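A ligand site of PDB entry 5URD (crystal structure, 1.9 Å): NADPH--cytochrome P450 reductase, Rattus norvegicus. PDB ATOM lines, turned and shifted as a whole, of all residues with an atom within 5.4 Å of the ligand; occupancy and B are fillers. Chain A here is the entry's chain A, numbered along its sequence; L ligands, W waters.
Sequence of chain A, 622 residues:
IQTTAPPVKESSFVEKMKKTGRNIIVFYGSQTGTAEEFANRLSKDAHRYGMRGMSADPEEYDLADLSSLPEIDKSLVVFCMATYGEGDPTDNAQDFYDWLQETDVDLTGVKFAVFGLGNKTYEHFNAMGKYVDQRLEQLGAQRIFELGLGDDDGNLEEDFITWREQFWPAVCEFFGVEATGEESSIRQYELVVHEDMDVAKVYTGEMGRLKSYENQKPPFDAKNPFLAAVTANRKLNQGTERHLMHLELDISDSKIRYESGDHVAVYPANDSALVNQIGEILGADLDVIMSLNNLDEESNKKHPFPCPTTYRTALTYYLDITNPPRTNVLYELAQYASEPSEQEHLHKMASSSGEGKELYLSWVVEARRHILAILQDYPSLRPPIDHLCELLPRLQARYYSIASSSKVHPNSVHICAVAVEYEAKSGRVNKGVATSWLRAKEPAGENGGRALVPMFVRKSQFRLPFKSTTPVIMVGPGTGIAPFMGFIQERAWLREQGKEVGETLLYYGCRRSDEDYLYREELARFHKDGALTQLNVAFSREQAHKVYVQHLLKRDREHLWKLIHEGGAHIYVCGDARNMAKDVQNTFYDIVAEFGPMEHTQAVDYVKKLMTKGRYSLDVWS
O5 of the ligand sits close to O of Cys 510, at 3.2 Å.
The side-chain hydroxyl of Ser 540 sits at hydrogen-bond distance from an oxygen (O13) of the ligand (2.7 Å).
O8 of the ligand sits at hydrogen-bond distance from OG1 of Thr 479, at 2.9 Å.
The backbone NH (N) of Thr 479 lies within hydrogen-bond range of an oxygen (O8) of the ligand, 2.7 Å away.
The guanidinium group of Arg 511 lies within salt-bridge range of an oxygen (O1) of the ligand (3.7 Å).
The guanidinium group (NE) of Arg 541 lies within salt-bridge range of an oxygen (O13) of the ligand (2.8 Å).
NZ of Lys 546 lies within salt-bridge range of O13 of the ligand (3.0 Å).
The side-chain carboxylate (OD2) of Asp 583 lies within hydrogen-bond range of a nitrogen (N3) of the ligand (3.1 Å).
OH of Tyr 548 sits at hydrogen-bond distance from O12 of the ligand, 2.6 Å away.
The guanidinium group of Arg 242 lies within salt-bridge range of an oxygen (O1) of the ligand.
NE2 of Gln 550 sits at hydrogen-bond distance from N4 of the ligand, 3.1 Å away.
Merely in contact with the ligand: Met 580 (3.5 Å), Gly 478 (3.6 Å), Asn 579 (3.7 Å), Pro 477 (3.8 Å) and Gly 509 (3.9 Å).
Hydrophobic or aromatic side chains that line the ligand: Pro 477, Tyr 548 and Met 580.
The guanidinium group (NH1) of Arg 242 is in salt-bridge range of the side-chain carboxylate (OD2) of Asp 516 (3.3 Å).
The backbone NH of Arg 541 is in hydrogen-bond range of the backbone carbonyl oxygen of Arg 511.
The backbone NH (N) of Ser 540 is in hydrogen-bond range of the backbone carbonyl oxygen (O) of Cys 510 (2.9 Å).
The side-chain carboxylate of Asp 516 lies within salt-bridge range of the guanidinium group of Arg 511, 3.9 Å away.
The backbone carbonyl oxygen of Ala 538 lies within hydrogen-bond range of the backbone NH of Cys 510 (3.1 Å).
The side-chain carboxylate of Asp 576 sits at hydrogen-bond distance from the backbone NH of Asn 579 (2.7 Å).
N of Met 580 is in hydrogen-bond range of OD2 of Asp 576 (3.0 Å).
The backbone NH of Gly 478 lies within hydrogen-bond range of the backbone carbonyl oxygen of Gly 509, 2.8 Å away.
Water W4 lies within hydrogen-bond range of an oxygen (O9) of the ligand (2.6 Å), the side-chain hydroxyl (OG1) of Thr 479 (3.3 Å) and the backbone NH (N) of Asp 576 (3.5 Å).
Water W6 lies within hydrogen-bond range of an oxygen (O1) of the ligand, the side-chain carboxylate of Asp 516 and the backbone NH of Arg 511.
Water W3 lies within hydrogen-bond range of a nitrogen (N5) of the ligand (2.9 Å) and the backbone NH of Val 549 (3.0 Å).
Water W7 bridges O5 of the ligand (2.9 Å) and O of Ala 538 (2.9 Å).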
ATOM      1  N   ARG A 242      11.484 -18.670  39.646  1.00  0.00           N
ATOM      2  CA  ARG A 242      10.238 -18.217  40.231  1.00  0.00           C
ATOM      3  C   ARG A 242       9.406 -19.405  40.712  1.00  0.00           C
ATOM      4  O   ARG A 242       9.835 -20.561  40.630  1.00  0.00           O
ATOM      5  CB  ARG A 242       9.428 -17.459  39.179  1.00  0.00           C
ATOM      6  CG  ARG A 242      10.271 -16.542  38.306  1.00  0.00           C
ATOM      7  CD  ARG A 242       9.689 -16.482  36.898  1.00  0.00           C
ATOM      8  NE  ARG A 242       8.564 -15.578  36.811  1.00  0.00           N
ATOM      9  CZ  ARG A 242       7.713 -15.523  35.802  1.00  0.00           C
ATOM     10  NH1 ARG A 242       7.848 -16.336  34.753  1.00  0.00           N
ATOM     11  NH2 ARG A 242       6.738 -14.632  35.807  1.00  0.00           N
ATOM     12  N   LEU A 244       5.623 -20.934  40.140  1.00  0.00           N
ATOM     13  CA  LEU A 244       4.324 -20.923  39.490  1.00  0.00           C
ATOM     14  C   LEU A 244       3.583 -22.134  40.005  1.00  0.00           C
ATOM     15  O   LEU A 244       4.126 -23.248  40.044  1.00  0.00           O
ATOM     16  CB  LEU A 244       4.462 -20.937  37.974  1.00  0.00           C
ATOM     17  CG  LEU A 244       4.982 -19.566  37.522  1.00  0.00           C
ATOM     18  CD1 LEU A 244       6.415 -19.687  37.074  1.00  0.00           C
ATOM     19  CD2 LEU A 244       4.095 -19.000  36.423  1.00  0.00           C
ATOM     20  N   VAL A 418       1.234 -17.129  39.549  1.00  0.00           N
ATOM     21  CA  VAL A 418       2.654 -16.932  39.821  1.00  0.00           C
ATOM     22  C   VAL A 418       2.765 -16.263  41.186  1.00  0.00           C
ATOM     23  O   VAL A 418       2.071 -15.276  41.466  1.00  0.00           O
ATOM     24  CB  VAL A 418       3.342 -16.072  38.715  1.00  0.00           C
ATOM     25  CG1 VAL A 418       2.610 -14.749  38.519  1.00  0.00           C
ATOM     26  CG2 VAL A 418       4.798 -15.828  39.074  1.00  0.00           C
ATOM     27  N   PRO A 477       0.479 -15.934  26.807  1.00  0.00           N
ATOM     28  CA  PRO A 477       1.811 -16.254  27.320  1.00  0.00           C
ATOM     29  C   PRO A 477       1.859 -16.196  28.854  1.00  0.00           C
ATOM     30  O   PRO A 477       1.081 -15.483  29.485  1.00  0.00           O
ATOM     31  CB  PRO A 477       2.699 -15.205  26.651  1.00  0.00           C
ATOM     32  CG  PRO A 477       1.785 -14.027  26.514  1.00  0.00           C
ATOM     33  CD  PRO A 477       0.490 -14.671  26.054  1.00  0.00           C
ATOM     34  N   GLY A 478       2.782 -16.950  29.441  1.00  0.00           N
ATOM     35  CA  GLY A 478       2.904 -16.973  30.883  1.00  0.00           C
ATOM     36  C   GLY A 478       1.617 -17.437  31.548  1.00  0.00           C
ATOM     37  O   GLY A 478       0.959 -18.355  31.042  1.00  0.00           O
ATOM     38  N   THR A 479       1.241 -16.794  32.650  1.00  0.00           N
ATOM     39  CA  THR A 479       0.023 -17.181  33.344  1.00  0.00           C
ATOM     40  C   THR A 479      -1.222 -16.876  32.512  1.00  0.00           C
ATOM     41  O   THR A 479      -2.338 -17.187  32.928  1.00  0.00           O
ATOM     42  CB  THR A 479      -0.098 -16.489  34.725  1.00  0.00           C
ATOM     43  OG1 THR A 479      -0.072 -15.065  34.565  1.00  0.00           O
ATOM     44  CG2 THR A 479       1.041 -16.935  35.647  1.00  0.00           C
ATOM     45  N   GLY A 480      -1.030 -16.279  31.342  1.00  0.00           N
ATOM     46  CA  GLY A 480      -2.153 -15.985  30.469  1.00  0.00           C
ATOM     47  C   GLY A 480      -2.724 -17.284  29.928  1.00  0.00           C
ATOM     48  O   GLY A 480      -3.795 -17.297  29.323  1.00  0.00           O
ATOM     49  N   GLY A 509       3.589 -18.752  25.459  1.00  0.00           N
ATOM     50  CA  GLY A 509       4.950 -18.279  25.570  1.00  0.00           C
ATOM     51  C   GLY A 509       5.514 -18.354  26.974  1.00  0.00           C
ATOM     52  O   GLY A 509       4.798 -18.136  27.947  1.00  0.00           O
ATOM     53  N   CYS A 510       6.786 -18.685  27.078  1.00  0.00           N
ATOM     54  CA  CYS A 510       7.458 -18.759  28.361  1.00  0.00           C
ATOM     55  C   CYS A 510       8.928 -18.450  28.112  1.00  0.00           C
ATOM     56  O   CYS A 510       9.334 -18.297  26.959  1.00  0.00           O
ATOM     57  CB  CYS A 510       7.301 -20.146  28.992  1.00  0.00           C
ATOM     58  SG  CYS A 510       8.066 -21.478  28.068  1.00  0.00           S
ATOM     59  N   ARG A 511       9.723 -18.361  29.165  1.00  0.00           N
ATOM     60  CA  ARG A 511      11.148 -18.043  29.034  1.00  0.00           C
ATOM     61  C   ARG A 511      11.981 -19.176  28.430  1.00  0.00           C
ATOM     62  O   ARG A 511      12.669 -18.968  27.431  1.00  0.00           O
ATOM     63  CB  ARG A 511      11.729 -17.665  30.402  1.00  0.00           C
ATOM     64  CG  ARG A 511      10.997 -16.512  31.066  1.00  0.00           C
ATOM     65  CD  ARG A 511      11.646 -16.171  32.410  1.00  0.00           C
ATOM     66  NE  ARG A 511      10.960 -15.058  33.054  1.00  0.00           N
ATOM     67  CZ  ARG A 511      11.343 -14.513  34.210  1.00  0.00           C
ATOM     68  NH1 ARG A 511      10.666 -13.499  34.715  1.00  0.00           N
ATOM     69  NH2 ARG A 511      12.411 -14.986  34.841  1.00  0.00           N
ATOM     70  N   ASP A 516      10.101 -22.557  32.860  1.00  0.00           N
ATOM     71  CA  ASP A 516       8.715 -22.257  33.205  1.00  0.00           C
ATOM     72  C   ASP A 516       7.675 -22.539  32.106  1.00  0.00           C
ATOM     73  O   ASP A 516       6.781 -21.716  31.866  1.00  0.00           O
ATOM     74  CB  ASP A 516       8.604 -20.804  33.654  1.00  0.00           C
ATOM     75  CG  ASP A 516       9.273 -19.835  32.690  1.00  0.00           C
ATOM     76  OD1 ASP A 516       9.615 -20.248  31.557  1.00  0.00           O
ATOM     77  OD2 ASP A 516       9.452 -18.652  33.059  1.00  0.00           O
ATOM     78  N   ALA A 538       6.426 -19.856  22.075  1.00  0.00           N
ATOM     79  CA  ALA A 538       7.507 -18.899  21.907  1.00  0.00           C
ATOM     80  C   ALA A 538       8.384 -18.933  23.152  1.00  0.00           C
ATOM     81  O   ALA A 538       7.945 -18.558  24.232  1.00  0.00           O
ATOM     82  CB  ALA A 538       6.939 -17.493  21.699  1.00  0.00           C
ATOM     83  N   SER A 540      10.999 -17.176  24.807  1.00  0.00           N
ATOM     84  CA  SER A 540      11.633 -15.866  24.740  1.00  0.00           C
ATOM     85  C   SER A 540      13.111 -15.780  25.062  1.00  0.00           C
ATOM     86  O   SER A 540      13.793 -14.891  24.551  1.00  0.00           O
ATOM     87  CB  SER A 540      10.872 -14.871  25.621  1.00  0.00           C
ATOM     88  OG  SER A 540      10.975 -15.187  27.003  1.00  0.00           O
ATOM     89  N   ARG A 541      13.629 -16.699  25.881  1.00  0.00           N
ATOM     90  CA  ARG A 541      15.043 -16.631  26.252  1.00  0.00           C
ATOM     91  C   ARG A 541      15.921 -17.784  25.817  1.00  0.00           C
ATOM     92  O   ARG A 541      17.006 -17.981  26.363  1.00  0.00           O
ATOM     93  CB  ARG A 541      15.147 -16.430  27.763  1.00  0.00           C
ATOM     94  CG  ARG A 541      14.277 -15.297  28.259  1.00  0.00           C
ATOM     95  CD  ARG A 541      14.460 -14.986  29.730  1.00  0.00           C
ATOM     96  NE  ARG A 541      13.544 -13.913  30.141  1.00  0.00           N
ATOM     97  CZ  ARG A 541      13.507 -13.390  31.354  1.00  0.00           C
ATOM     98  NH1 ARG A 541      14.339 -13.828  32.294  1.00  0.00           N
ATOM     99  NH2 ARG A 541      12.632 -12.439  31.636  1.00  0.00           N
ATOM    100  N   LYS A 546      14.472 -11.912  21.301  1.00  0.00           N
ATOM    101  CA  LYS A 546      13.226 -12.290  21.944  1.00  0.00           C
ATOM    102  C   LYS A 546      12.322 -12.939  20.918  1.00  0.00           C
ATOM    103  O   LYS A 546      12.254 -12.492  19.776  1.00  0.00           O
ATOM    104  CB  LYS A 546      12.503 -11.053  22.501  1.00  0.00           C
ATOM    105  CG  LYS A 546      13.240 -10.326  23.600  1.00  0.00           C
ATOM    106  CD  LYS A 546      13.358 -11.192  24.843  1.00  0.00           C
ATOM    107  CE  LYS A 546      13.967 -10.427  26.004  1.00  0.00           C
ATOM    108  NZ  LYS A 546      14.106 -11.306  27.194  1.00  0.00           N
ATOM    109  N   TYR A 548       8.420 -13.907  20.834  1.00  0.00           N
ATOM    110  CA  TYR A 548       7.162 -13.759  21.543  1.00  0.00           C
ATOM    111  C   TYR A 548       5.993 -14.322  20.739  1.00  0.00           C
ATOM    112  O   TYR A 548       6.124 -14.590  19.555  1.00  0.00           O
ATOM    113  CB  TYR A 548       6.889 -12.284  21.836  1.00  0.00           C
ATOM    114  CG  TYR A 548       7.863 -11.603  22.787  1.00  0.00           C
ATOM    115  CD1 TYR A 548       8.415 -12.292  23.881  1.00  0.00           C
ATOM    116  CD2 TYR A 548       8.157 -10.247  22.647  1.00  0.00           C
ATOM    117  CE1 TYR A 548       9.220 -11.629  24.816  1.00  0.00           C
ATOM    118  CE2 TYR A 548       8.962  -9.584  23.581  1.00  0.00           C
ATOM    119  CZ  TYR A 548       9.482 -10.287  24.653  1.00  0.00           C
ATOM    120  OH  TYR A 548      10.238  -9.601  25.589  1.00  0.00           O
ATOM    121  N   VAL A 549       4.846 -14.463  21.388  1.00  0.00           N
ATOM    122  CA  VAL A 549       3.689 -15.013  20.708  1.00  0.00           C
ATOM    123  C   VAL A 549       3.334 -14.222  19.451  1.00  0.00           C
ATOM    124  O   VAL A 549       2.969 -14.819  18.448  1.00  0.00           O
ATOM    125  CB  VAL A 549       2.442 -15.114  21.660  1.00  0.00           C
ATOM    126  CG1 VAL A 549       2.662 -16.216  22.684  1.00  0.00           C
ATOM    127  CG2 VAL A 549       2.160 -13.774  22.354  1.00  0.00           C
ATOM    128  N   GLN A 550       3.450 -12.890  19.474  1.00  0.00           N
ATOM    129  CA  GLN A 550       3.114 -12.103  18.287  1.00  0.00           C
ATOM    130  C   GLN A 550       4.023 -12.409  17.097  1.00  0.00           C
ATOM    131  O   GLN A 550       3.617 -12.228  15.942  1.00  0.00           O
ATOM    132  CB  GLN A 550       3.145 -10.596  18.588  1.00  0.00           C
ATOM    133  CG  GLN A 550       4.459 -10.097  19.147  1.00  0.00           C
ATOM    134  CD  GLN A 550       4.432  -9.991  20.649  1.00  0.00           C
ATOM    135  OE1 GLN A 550       3.845 -10.832  21.337  1.00  0.00           O
ATOM    136  NE2 GLN A 550       5.070  -8.959  21.185  1.00  0.00           N
ATOM    137  N   ASP A 576      -0.776 -10.315  30.259  1.00  0.00           N
ATOM    138  CA  ASP A 576      -0.331  -8.952  30.494  1.00  0.00           C
ATOM    139  C   ASP A 576      -1.053  -7.895  29.666  1.00  0.00           C
ATOM    140  O   ASP A 576      -0.933  -7.878  28.444  1.00  0.00           O
ATOM    141  CB  ASP A 576       1.176  -8.840  30.244  1.00  0.00           C
ATOM    142  CG  ASP A 576       1.656  -7.408  30.343  1.00  0.00           C
ATOM    143  OD1 ASP A 576       1.415  -6.773  31.404  1.00  0.00           O
ATOM    144  OD2 ASP A 576       2.259  -6.917  29.371  1.00  0.00           O
ATOM    145  N   ASN A 579       1.833  -4.531  28.105  1.00  0.00           N
ATOM    146  CA  ASN A 579       2.527  -4.565  26.831  1.00  0.00           C
ATOM    147  C   ASN A 579       2.108  -5.680  25.857  1.00  0.00           C
ATOM    148  O   ASN A 579       1.902  -5.414  24.672  1.00  0.00           O
ATOM    149  CB  ASN A 579       4.036  -4.659  27.050  1.00  0.00           C
ATOM    150  CG  ASN A 579       4.591  -3.442  27.800  1.00  0.00           C
ATOM    151  OD1 ASN A 579       4.502  -3.337  29.018  1.00  0.00           O
ATOM    152  ND2 ASN A 579       5.177  -2.512  27.055  1.00  0.00           N
ATOM    153  N   MET A 580       2.010  -6.906  26.356  1.00  0.00           N
ATOM    154  CA  MET A 580       1.672  -8.029  25.499  1.00  0.00           C
ATOM    155  C   MET A 580       0.372  -7.847  24.721  1.00  0.00           C
ATOM    156  O   MET A 580       0.368  -7.951  23.498  1.00  0.00           O
ATOM    157  CB  MET A 580       1.613  -9.321  26.322  1.00  0.00           C
ATOM    158  CG  MET A 580       1.341 -10.587  25.512  1.00  0.00           C
ATOM    159  SD  MET A 580      -0.411 -10.853  25.106  1.00  0.00           S
ATOM    160  CE  MET A 580      -1.099 -11.143  26.750  1.00  0.00           C
ATOM    161  N   ASP A 583       0.800  -5.326  21.917  1.00  0.00           N
ATOM    162  CA  ASP A 583       1.693  -5.788  20.849  1.00  0.00           C
ATOM    163  C   ASP A 583       0.984  -6.837  19.988  1.00  0.00           C
ATOM    164  O   ASP A 583       1.178  -6.895  18.784  1.00  0.00           O
ATOM    165  CB  ASP A 583       2.987  -6.381  21.435  1.00  0.00           C
ATOM    166  CG  ASP A 583       3.906  -5.321  22.013  1.00  0.00           C
ATOM    167  OD1 ASP A 583       3.839  -4.152  21.571  1.00  0.00           O
ATOM    168  OD2 ASP A 583       4.719  -5.660  22.905  1.00  0.00           O
HETATM  169  P1  LIG L   1       6.319 -13.780  32.267  1.00  0.00           P
HETATM  170  O1  LIG L   1       7.329 -14.852  32.339  1.00  0.00           O
HETATM  171  O2  LIG L   1       6.622 -12.469  32.874  1.00  0.00           O
HETATM  172  O3  LIG L   1       5.898 -13.561  30.725  1.00  0.00           O
HETATM  173  C1  LIG L   1       5.550 -14.680  29.918  1.00  0.00           C
HETATM  174  C2  LIG L   1       6.213 -14.582  28.547  1.00  0.00           C
HETATM  175  O4  LIG L   1       5.813 -13.362  27.911  1.00  0.00           O
HETATM  176  C3  LIG L   1       7.737 -14.526  28.690  1.00  0.00           C
HETATM  177  O5  LIG L   1       8.348 -15.330  27.670  1.00  0.00           O
HETATM  178  C4  LIG L   1       8.048 -13.051  28.447  1.00  0.00           C
HETATM  179  O6  LIG L   1       9.346 -12.955  27.862  1.00  0.00           O
HETATM  180  C5  LIG L   1       7.016 -12.786  27.372  1.00  0.00           C
HETATM  181  N1  LIG L   1       6.829 -11.344  27.074  1.00  0.00           N
HETATM  182  C6  LIG L   1       7.359 -10.315  27.731  1.00  0.00           C
HETATM  183  N2  LIG L   1       6.944  -9.204  27.135  1.00  0.00           N
HETATM  184  C7  LIG L   1       6.166  -9.538  26.108  1.00  0.00           C
HETATM  185  C8  LIG L   1       5.527  -8.802  25.204  1.00  0.00           C
HETATM  186  N3  LIG L   1       5.709  -7.482  25.247  1.00  0.00           N
HETATM  187  N4  LIG L   1       4.766  -9.365  24.252  1.00  0.00           N
HETATM  188  C9  LIG L   1       4.628 -10.758  24.223  1.00  0.00           C
HETATM  189  N5  LIG L   1       5.315 -11.497  25.186  1.00  0.00           N
HETATM  190  C10 LIG L   1       6.070 -10.863  26.093  1.00  0.00           C
HETATM  191  O7  LIG L   1       4.958 -14.335  32.929  1.00  0.00           O
HETATM  192  P2  LIG L   1       3.653 -13.793  33.687  1.00  0.00           P
HETATM  193  O8  LIG L   1       2.719 -14.912  33.924  1.00  0.00           O
HETATM  194  O9  LIG L   1       3.171 -12.602  32.953  1.00  0.00           O
HETATM  195  O10 LIG L   1       4.245 -13.319  35.109  1.00  0.00           O
HETATM  196  P3  LIG L   1      10.566 -12.132  28.546  1.00  0.00           P
HETATM  197  O11 LIG L   1      10.242 -12.146  29.995  1.00  0.00           O
HETATM  198  O12 LIG L   1      10.491 -10.806  27.904  1.00  0.00           O
HETATM  199  O13 LIG L   1      11.753 -12.932  28.175  1.00  0.00           O
HETATM  200  O   HOH W   1       8.670 -10.834  31.373  1.00  0.00           O
HETATM  201  O   HOH W   2       3.557 -11.456  28.566  1.00  0.00           O
HETATM  202  O   HOH W   3       5.203 -14.252  24.325  1.00  0.00           O
HETATM  203  O   HOH W   4       0.623 -12.679  32.407  1.00  0.00           O
HETATM  204  O   HOH W   5       7.535  -5.323  26.114  1.00  0.00           O
HETATM  205  O   HOH W   6       7.377 -17.366  31.431  1.00  0.00           O
HETATM  206  O   HOH W   7       7.282 -15.824  25.013  1.00  0.00           O
HETATM  207  O   HOH W   8      11.182  -8.630  29.119  1.00  0.00           O
